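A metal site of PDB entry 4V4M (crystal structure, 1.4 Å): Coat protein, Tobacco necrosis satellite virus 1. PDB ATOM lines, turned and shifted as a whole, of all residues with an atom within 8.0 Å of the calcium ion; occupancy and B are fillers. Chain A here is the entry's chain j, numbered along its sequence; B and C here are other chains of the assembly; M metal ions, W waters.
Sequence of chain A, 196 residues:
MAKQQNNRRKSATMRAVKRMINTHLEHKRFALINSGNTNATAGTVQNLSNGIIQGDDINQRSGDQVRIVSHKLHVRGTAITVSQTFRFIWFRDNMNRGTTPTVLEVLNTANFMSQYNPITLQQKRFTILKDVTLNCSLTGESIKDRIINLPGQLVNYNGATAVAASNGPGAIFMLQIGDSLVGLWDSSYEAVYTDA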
ATOM      1  N   LYS A  28     -14.709  22.404  24.884  1.00  0.00           N
ATOM      2  CA  LYS A  28     -14.336  22.130  23.521  1.00  0.00           C
ATOM      3  C   LYS A  28     -13.183  23.047  23.132  1.00  0.00           C
ATOM      4  O   LYS A  28     -12.868  24.029  23.834  1.00  0.00           O
ATOM      5  CB  LYS A  28     -15.553  22.297  22.617  1.00  0.00           C
ATOM      6  CG  LYS A  28     -16.604  21.195  22.820  1.00  0.00           C
ATOM      7  CD  LYS A  28     -17.776  21.266  21.805  1.00  0.00           C
ATOM      8  CE  LYS A  28     -18.867  20.223  22.127  1.00  0.00           C
ATOM      9  NZ  LYS A  28     -20.054  20.277  21.232  1.00  0.00           N
ATOM     10  N   GLN A  60     -16.088  21.563  17.027  1.00  0.00           N
ATOM     11  CA  GLN A  60     -17.335  21.991  16.382  1.00  0.00           C
ATOM     12  C   GLN A  60     -18.364  22.470  17.411  1.00  0.00           C
ATOM     13  O   GLN A  60     -18.029  22.633  18.585  1.00  0.00           O
ATOM     14  CB  GLN A  60     -17.877  20.853  15.520  1.00  0.00           C
ATOM     15  CG  GLN A  60     -16.882  20.484  14.428  1.00  0.00           C
ATOM     16  CD  GLN A  60     -17.309  19.323  13.578  1.00  0.00           C
ATOM     17  OE1 GLN A  60     -17.922  18.357  14.048  1.00  0.00           O
ATOM     18  NE2 GLN A  60     -16.931  19.383  12.313  1.00  0.00           N
ATOM     19  N   ARG A  61     -19.596  22.697  16.971  1.00  0.00           N
ATOM     20  CA  ARG A  61     -20.621  23.252  17.862  1.00  0.00           C
ATOM     21  C   ARG A  61     -22.005  22.690  17.592  1.00  0.00           C
ATOM     22  O   ARG A  61     -22.326  22.304  16.463  1.00  0.00           O
ATOM     23  CB  ARG A  61     -20.688  24.777  17.759  1.00  0.00           C
ATOM     24  CG  ARG A  61     -21.008  25.275  16.339  1.00  0.00           C
ATOM     25  CD  ARG A  61     -21.028  26.809  16.252  1.00  0.00           C
ATOM     26  NE  ARG A  61     -20.825  27.245  14.875  1.00  0.00           N
ATOM     27  CZ  ARG A  61     -21.792  27.577  14.013  1.00  0.00           C
ATOM     28  NH1 ARG A  61     -23.078  27.532  14.351  1.00  0.00           N
ATOM     29  NH2 ARG A  61     -21.444  27.966  12.792  1.00  0.00           N
ATOM     30  N   SER A  62     -22.803  22.612  18.639  1.00  0.00           N
ATOM     31  CA  SER A  62     -24.232  22.355  18.511  1.00  0.00           C
ATOM     32  C   SER A  62     -24.942  23.718  18.506  1.00  0.00           C
ATOM     33  O   SER A  62     -24.613  24.578  19.315  1.00  0.00           O
ATOM     34  CB  SER A  62     -24.721  21.575  19.743  1.00  0.00           C
ATOM     35  OG  SER A  62     -26.052  21.149  19.577  1.00  0.00           O
ATOM     36  N   GLY A  63     -25.900  23.919  17.603  1.00  0.00           N
ATOM     37  CA  GLY A  63     -26.619  25.192  17.565  1.00  0.00           C
ATOM     38  C   GLY A  63     -25.781  26.370  17.071  1.00  0.00           C
ATOM     39  O   GLY A  63     -24.764  26.194  16.405  1.00  0.00           O
ATOM     40  N   ASP A  64     -26.231  27.570  17.406  1.00  0.00           N
ATOM     41  CA  ASP A  64     -25.651  28.789  16.856  1.00  0.00           C
ATOM     42  C   ASP A  64     -25.024  29.671  17.941  1.00  0.00           C
ATOM     43  O   ASP A  64     -24.800  30.873  17.719  1.00  0.00           O
ATOM     44  CB  ASP A  64     -26.711  29.566  16.062  1.00  0.00           C
ATOM     45  CG  ASP A  64     -26.877  29.056  14.643  1.00  0.00           C
ATOM     46  OD1 ASP A  64     -25.945  28.382  14.101  1.00  0.00           O
ATOM     47  OD2 ASP A  64     -27.950  29.339  14.048  1.00  0.00           O
ATOM     48  N   GLN A  65     -24.718  29.073  19.105  1.00  0.00           N
ATOM     49  CA  GLN A  65     -23.999  29.797  20.171  1.00  0.00           C
ATOM     50  C   GLN A  65     -22.904  28.925  20.767  1.00  0.00           C
ATOM     51  O   GLN A  65     -23.063  27.731  20.926  1.00  0.00           O
ATOM     52  CB  GLN A  65     -24.939  30.217  21.296  1.00  0.00           C
ATOM     53  CG  GLN A  65     -25.851  31.349  20.942  1.00  0.00           C
ATOM     54  CD  GLN A  65     -26.586  31.871  22.162  1.00  0.00           C
ATOM     55  OE1 GLN A  65     -26.733  31.176  23.174  1.00  0.00           O
ATOM     56  NE2 GLN A  65     -27.059  33.111  22.073  1.00  0.00           N
ATOM     57  N   VAL A  66     -21.773  29.556  21.080  1.00  0.00           N
ATOM     58  CA  VAL A  66     -20.791  28.972  21.985  1.00  0.00           C
ATOM     59  C   VAL A  66     -20.356  30.066  22.956  1.00  0.00           C
ATOM     60  O   VAL A  66     -20.662  31.247  22.745  1.00  0.00           O
ATOM     61  CB  VAL A  66     -19.552  28.386  21.264  1.00  0.00           C
ATOM     62  CG1 VAL A  66     -19.968  27.303  20.257  1.00  0.00           C
ATOM     63  CG2 VAL A  66     -18.766  29.498  20.589  1.00  0.00           C
ATOM     64  N   ARG A  67     -19.661  29.688  24.023  1.00  0.00           N
ATOM     65  CA  ARG A  67     -19.121  30.669  24.974  1.00  0.00           C
ATOM     66  C   ARG A  67     -17.627  30.438  25.105  1.00  0.00           C
ATOM     67  O   ARG A  67     -17.197  29.435  25.658  1.00  0.00           O
ATOM     68  CB  ARG A  67     -19.789  30.549  26.342  1.00  0.00           C
ATOM     69  CG  ARG A  67     -19.311  31.594  27.343  1.00  0.00           C
ATOM     70  CD  ARG A  67     -20.180  31.651  28.602  1.00  0.00           C
ATOM     71  NE  ARG A  67     -21.513  32.158  28.316  1.00  0.00           N
ATOM     72  CZ  ARG A  67     -21.849  33.450  28.286  1.00  0.00           C
ATOM     73  NH1 ARG A  67     -20.941  34.387  28.527  1.00  0.00           N
ATOM     74  NH2 ARG A  67     -23.090  33.806  28.004  1.00  0.00           N
ATOM     75  N   LEU A 154     -19.480  35.236  24.837  1.00  0.00           N
ATOM     76  CA  LEU A 154     -20.477  34.625  23.937  1.00  0.00           C
ATOM     77  C   LEU A 154     -20.143  34.884  22.467  1.00  0.00           C
ATOM     78  O   LEU A 154     -19.759  36.001  22.098  1.00  0.00           O
ATOM     79  CB  LEU A 154     -21.858  35.226  24.214  1.00  0.00           C
ATOM     80  CG  LEU A 154     -23.053  34.710  23.418  1.00  0.00           C
ATOM     81  CD1 LEU A 154     -23.248  33.218  23.642  1.00  0.00           C
ATOM     82  CD2 LEU A 154     -24.318  35.476  23.833  1.00  0.00           C
ATOM     83  N   VAL A 155     -20.283  33.851  21.637  1.00  0.00           N
ATOM     84  CA  VAL A 155     -20.226  34.002  20.184  1.00  0.00           C
ATOM     85  C   VAL A 155     -21.531  33.463  19.594  1.00  0.00           C
ATOM     86  O   VAL A 155     -21.877  32.302  19.844  1.00  0.00           O
ATOM     87  CB  VAL A 155     -19.041  33.215  19.532  1.00  0.00           C
ATOM     88  CG1 VAL A 155     -18.969  33.491  18.045  1.00  0.00           C
ATOM     89  CG2 VAL A 155     -17.712  33.582  20.155  1.00  0.00           C
ATOM     90  N   TYR A 157     -23.741  32.770  15.976  1.00  0.00           N
ATOM     91  CA  TYR A 157     -23.558  32.477  14.562  1.00  0.00           C
ATOM     92  C   TYR A 157     -24.856  32.677  13.794  1.00  0.00           C
ATOM     93  O   TYR A 157     -25.940  32.540  14.344  1.00  0.00           O
ATOM     94  CB  TYR A 157     -23.066  31.024  14.394  1.00  0.00           C
ATOM     95  CG  TYR A 157     -21.659  30.802  14.889  1.00  0.00           C
ATOM     96  CD1 TYR A 157     -21.400  30.576  16.244  1.00  0.00           C
ATOM     97  CD2 TYR A 157     -20.585  30.824  14.008  1.00  0.00           C
ATOM     98  CE1 TYR A 157     -20.086  30.395  16.703  1.00  0.00           C
ATOM     99  CE2 TYR A 157     -19.268  30.629  14.456  1.00  0.00           C
ATOM    100  CZ  TYR A 157     -19.037  30.417  15.803  1.00  0.00           C
ATOM    101  OH  TYR A 157     -17.715  30.247  16.213  1.00  0.00           O
ATOM    102  N   TYR A 193     -13.874  26.670  24.515  1.00  0.00           N
ATOM    103  CA  TYR A 193     -15.246  27.161  24.658  1.00  0.00           C
ATOM    104  C   TYR A 193     -16.190  26.121  25.216  1.00  0.00           C
ATOM    105  O   TYR A 193     -15.960  24.933  25.035  1.00  0.00           O
ATOM    106  CB  TYR A 193     -15.783  27.636  23.293  1.00  0.00           C
ATOM    107  CG  TYR A 193     -15.734  26.601  22.174  1.00  0.00           C
ATOM    108  CD1 TYR A 193     -14.561  26.372  21.468  1.00  0.00           C
ATOM    109  CD2 TYR A 193     -16.863  25.865  21.841  1.00  0.00           C
ATOM    110  CE1 TYR A 193     -14.511  25.435  20.454  1.00  0.00           C
ATOM    111  CE2 TYR A 193     -16.836  24.920  20.830  1.00  0.00           C
ATOM    112  CZ  TYR A 193     -15.654  24.713  20.118  1.00  0.00           C
ATOM    113  OH  TYR A 193     -15.598  23.784  19.106  1.00  0.00           O
ATOM    114  N   THR A 194     -17.252  26.563  25.905  1.00  0.00           N
ATOM    115  CA  THR A 194     -18.318  25.639  26.257  1.00  0.00           C
ATOM    116  C   THR A 194     -19.421  25.736  25.235  1.00  0.00           C
ATOM    117  O   THR A 194     -19.523  26.730  24.490  1.00  0.00           O
ATOM    118  CB  THR A 194     -18.884  25.894  27.642  1.00  0.00           C
ATOM    119  OG1 THR A 194     -19.426  27.225  27.697  1.00  0.00           O
ATOM    120  CG2 THR A 194     -17.777  25.732  28.680  1.00  0.00           C
ATOM    121  N   ASP A 195     -20.277  24.713  25.212  1.00  0.00           N
ATOM    122  CA  ASP A 195     -21.261  24.577  24.162  1.00  0.00           C
ATOM    123  C   ASP A 195     -22.494  23.862  24.714  1.00  0.00           C
ATOM    124  O   ASP A 195     -22.969  22.876  24.141  1.00  0.00           O
ATOM    125  CB  ASP A 195     -20.647  23.795  22.993  1.00  0.00           C
ATOM    126  CG  ASP A 195     -21.553  23.719  21.785  1.00  0.00           C
ATOM    127  OD1 ASP A 195     -21.459  22.704  21.061  1.00  0.00           O
ATOM    128  OD2 ASP A 195     -22.335  24.673  21.527  1.00  0.00           O
ATOM    129  N   ALA A 196     -23.002  24.377  25.827  1.00  0.00           N
ATOM    130  CA  ALA A 196     -24.104  23.748  26.544  1.00  0.00           C
ATOM    131  C   ALA A 196     -25.442  24.401  26.219  1.00  0.00           C
ATOM    132  O   ALA A 196     -26.477  23.912  26.666  1.00  0.00           O
ATOM    133  CB  ALA A 196     -23.856  23.808  28.050  1.00  0.00           C
ATOM    134  OXT ALA A 196     -25.537  25.412  25.520  1.00  0.00           O
ATOM    135  N   HIS B  24     -25.443  30.049  30.798  1.00  0.00           N
ATOM    136  CA  HIS B  24     -24.442  29.204  30.146  1.00  0.00           C
ATOM    137  C   HIS B  24     -25.051  28.277  29.104  1.00  0.00           C
ATOM    138  O   HIS B  24     -24.328  27.560  28.429  1.00  0.00           O
ATOM    139  CB  HIS B  24     -23.692  28.363  31.173  1.00  0.00           C
ATOM    140  CG  HIS B  24     -22.797  29.169  32.050  1.00  0.00           C
ATOM    141  ND1 HIS B  24     -21.527  29.538  31.665  1.00  0.00           N
ATOM    142  CD2 HIS B  24     -22.995  29.711  33.284  1.00  0.00           C
ATOM    143  CE1 HIS B  24     -20.969  30.262  32.629  1.00  0.00           C
ATOM    144  NE2 HIS B  24     -21.843  30.384  33.619  1.00  0.00           N
ATOM    145  N   LEU B  25     -26.374  28.285  29.015  1.00  0.00           N
ATOM    146  CA  LEU B  25     -27.083  27.362  28.122  1.00  0.00           C
ATOM    147  C   LEU B  25     -27.629  28.094  26.906  1.00  0.00           C
ATOM    148  O   LEU B  25     -28.308  29.113  27.045  1.00  0.00           O
ATOM    149  CB  LEU B  25     -28.230  26.679  28.872  1.00  0.00           C
ATOM    150  CG  LEU B  25     -27.906  25.976  30.200  1.00  0.00           C
ATOM    151  CD1 LEU B  25     -29.123  25.195  30.709  1.00  0.00           C
ATOM    152  CD2 LEU B  25     -26.708  25.056  30.055  1.00  0.00           C
ATOM    153  N   GLU B  26     -27.336  27.574  25.725  1.00  0.00           N
ATOM    154  CA  GLU B  26     -27.919  28.120  24.500  1.00  0.00           C
ATOM    155  C   GLU B  26     -29.440  27.981  24.534  1.00  0.00           C
ATOM    156  O   GLU B  26     -29.964  26.890  24.756  1.00  0.00           O
ATOM    157  CB  GLU B  26     -27.372  27.413  23.255  1.00  0.00           C
ATOM    158  CG  GLU B  26     -27.964  27.983  21.987  1.00  0.00           C
ATOM    159  CD  GLU B  26     -27.300  27.505  20.707  1.00  0.00           C
ATOM    160  OE1 GLU B  26     -26.195  26.936  20.735  1.00  0.00           O
ATOM    161  OE2 GLU B  26     -27.921  27.682  19.633  1.00  0.00           O
ATOM    162  N   HIS B  27     -30.140  29.085  24.307  1.00  0.00           N
ATOM    163  CA  HIS B  27     -31.579  29.039  24.123  1.00  0.00           C
ATOM    164  C   HIS B  27     -31.860  28.862  22.637  1.00  0.00           C
ATOM    165  O   HIS B  27     -31.914  29.825  21.862  1.00  0.00           O
ATOM    166  CB  HIS B  27     -32.223  30.276  24.737  1.00  0.00           C
ATOM    167  CG  HIS B  27     -32.060  30.303  26.234  1.00  0.00           C
ATOM    168  ND1 HIS B  27     -33.071  30.648  27.097  1.00  0.00           N
ATOM    169  CD2 HIS B  27     -31.004  29.941  27.004  1.00  0.00           C
ATOM    170  CE1 HIS B  27     -32.638  30.534  28.338  1.00  0.00           C
ATOM    171  NE2 HIS B  27     -31.386  30.104  28.311  1.00  0.00           N
ATOM    172  N   LYS B  28     -31.976  27.602  22.245  1.00  0.00           N
ATOM    173  CA  LYS B  28     -32.358  27.217  20.886  1.00  0.00           C
ATOM    174  C   LYS B  28     -33.810  27.672  20.653  1.00  0.00           C
ATOM    175  O   LYS B  28     -34.524  28.005  21.587  1.00  0.00           O
ATOM    176  CB  LYS B  28     -32.167  25.714  20.713  1.00  0.00           C
ATOM    177  CG  LYS B  28     -30.675  25.289  20.699  1.00  0.00           C
ATOM    178  CD  LYS B  28     -30.481  23.822  20.352  1.00  0.00           C
ATOM    179  CE  LYS B  28     -28.983  23.490  20.338  1.00  0.00           C
ATOM    180  NZ  LYS B  28     -28.672  22.028  20.250  1.00  0.00           N
ATOM    181  N   ASP B  56     -27.877  19.335  14.537  1.00  0.00           N
ATOM    182  CA  ASP B  56     -26.944  20.303  15.116  1.00  0.00           C
ATOM    183  C   ASP B  56     -27.385  21.773  14.933  1.00  0.00           C
ATOM    184  O   ASP B  56     -26.674  22.678  15.352  1.00  0.00           O
ATOM    185  CB  ASP B  56     -25.544  20.123  14.486  1.00  0.00           C
ATOM    186  CG  ASP B  56     -25.046  18.706  14.577  1.00  0.00           C
ATOM    187  OD1 ASP B  56     -25.462  17.991  15.502  1.00  0.00           O
ATOM    188  OD2 ASP B  56     -24.243  18.308  13.717  1.00  0.00           O
ATOM    189  N   ASP B 195     -31.047  22.802  25.749  1.00  0.00           N
ATOM    190  CA  ASP B 195     -30.733  21.476  25.222  1.00  0.00           C
ATOM    191  C   ASP B 195     -29.365  21.015  25.744  1.00  0.00           C
ATOM    192  O   ASP B 195     -28.526  20.503  24.989  1.00  0.00           O
ATOM    193  CB  ASP B 195     -30.752  21.559  23.687  1.00  0.00           C
ATOM    194  CG  ASP B 195     -30.568  20.201  23.032  1.00  0.00           C
ATOM    195  OD1 ASP B 195     -29.946  20.117  21.945  1.00  0.00           O
ATOM    196  OD2 ASP B 195     -31.031  19.222  23.590  1.00  0.00           O
ATOM    197  N   GLN C 122     -32.566  35.027  18.737  1.00  0.00           N
ATOM    198  CA  GLN C 122     -31.638  34.366  19.680  1.00  0.00           C
ATOM    199  C   GLN C 122     -30.466  35.281  20.024  1.00  0.00           C
ATOM    200  O   GLN C 122     -30.092  35.410  21.197  1.00  0.00           O
ATOM    201  CB  GLN C 122     -31.093  33.056  19.123  1.00  0.00           C
ATOM    202  CG  GLN C 122     -30.008  32.448  20.036  1.00  0.00           C
ATOM    203  CD  GLN C 122     -29.281  31.252  19.410  1.00  0.00           C
ATOM    204  OE1 GLN C 122     -28.446  31.418  18.520  1.00  0.00           O
ATOM    205  NE2 GLN C 122     -29.566  30.046  19.896  1.00  0.00           N
HETATM  206 CA    CA M   1     -24.298  25.758  21.332  1.00  0.00          CA
HETATM  207  O   HOH W   1     -25.369  23.954  22.449  1.00  0.00           O
HETATM  208  O   HOH W   2     -24.112  26.539  23.532  1.00  0.00           O
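The side-chain carboxylate of Glu 26 of chain B is in hydrogen-bond range of the backbone NH of Asp 64 (2.8 Å). NZ of Lys 28 of chain B is in hydrogen-bond range of OG of Ser 62 (2.8 Å). NE2 of Gln 122 of chain C is in hydrogen-bond range of OE2 of Glu 26 of chain B (2.9 Å). NZ of Lys 28 of chain A lies within salt-bridge range of OD1 of Asp 195 of chain A, 2.8 Å away. OXT of Ala 196 sits at hydrogen-bond distance from N of Glu 26 of chain B, 2.8 Å away.
The calcium ion is bound by OD2 of Asp 195 of chain A (2.3 Å), OE1 of Glu 26 of chain B (2.3 Å), water W2 (2.3 Å), O of Ser 62 (2.4 Å), O of Gln 65 (2.4 Å) and water W1 (2.4 Å).
Water W1 bridges the backbone carbonyl oxygen of Asp 195 of chain A (3.1 Å) and the chain-end carboxylate of Ala 196 (3.4 Å).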
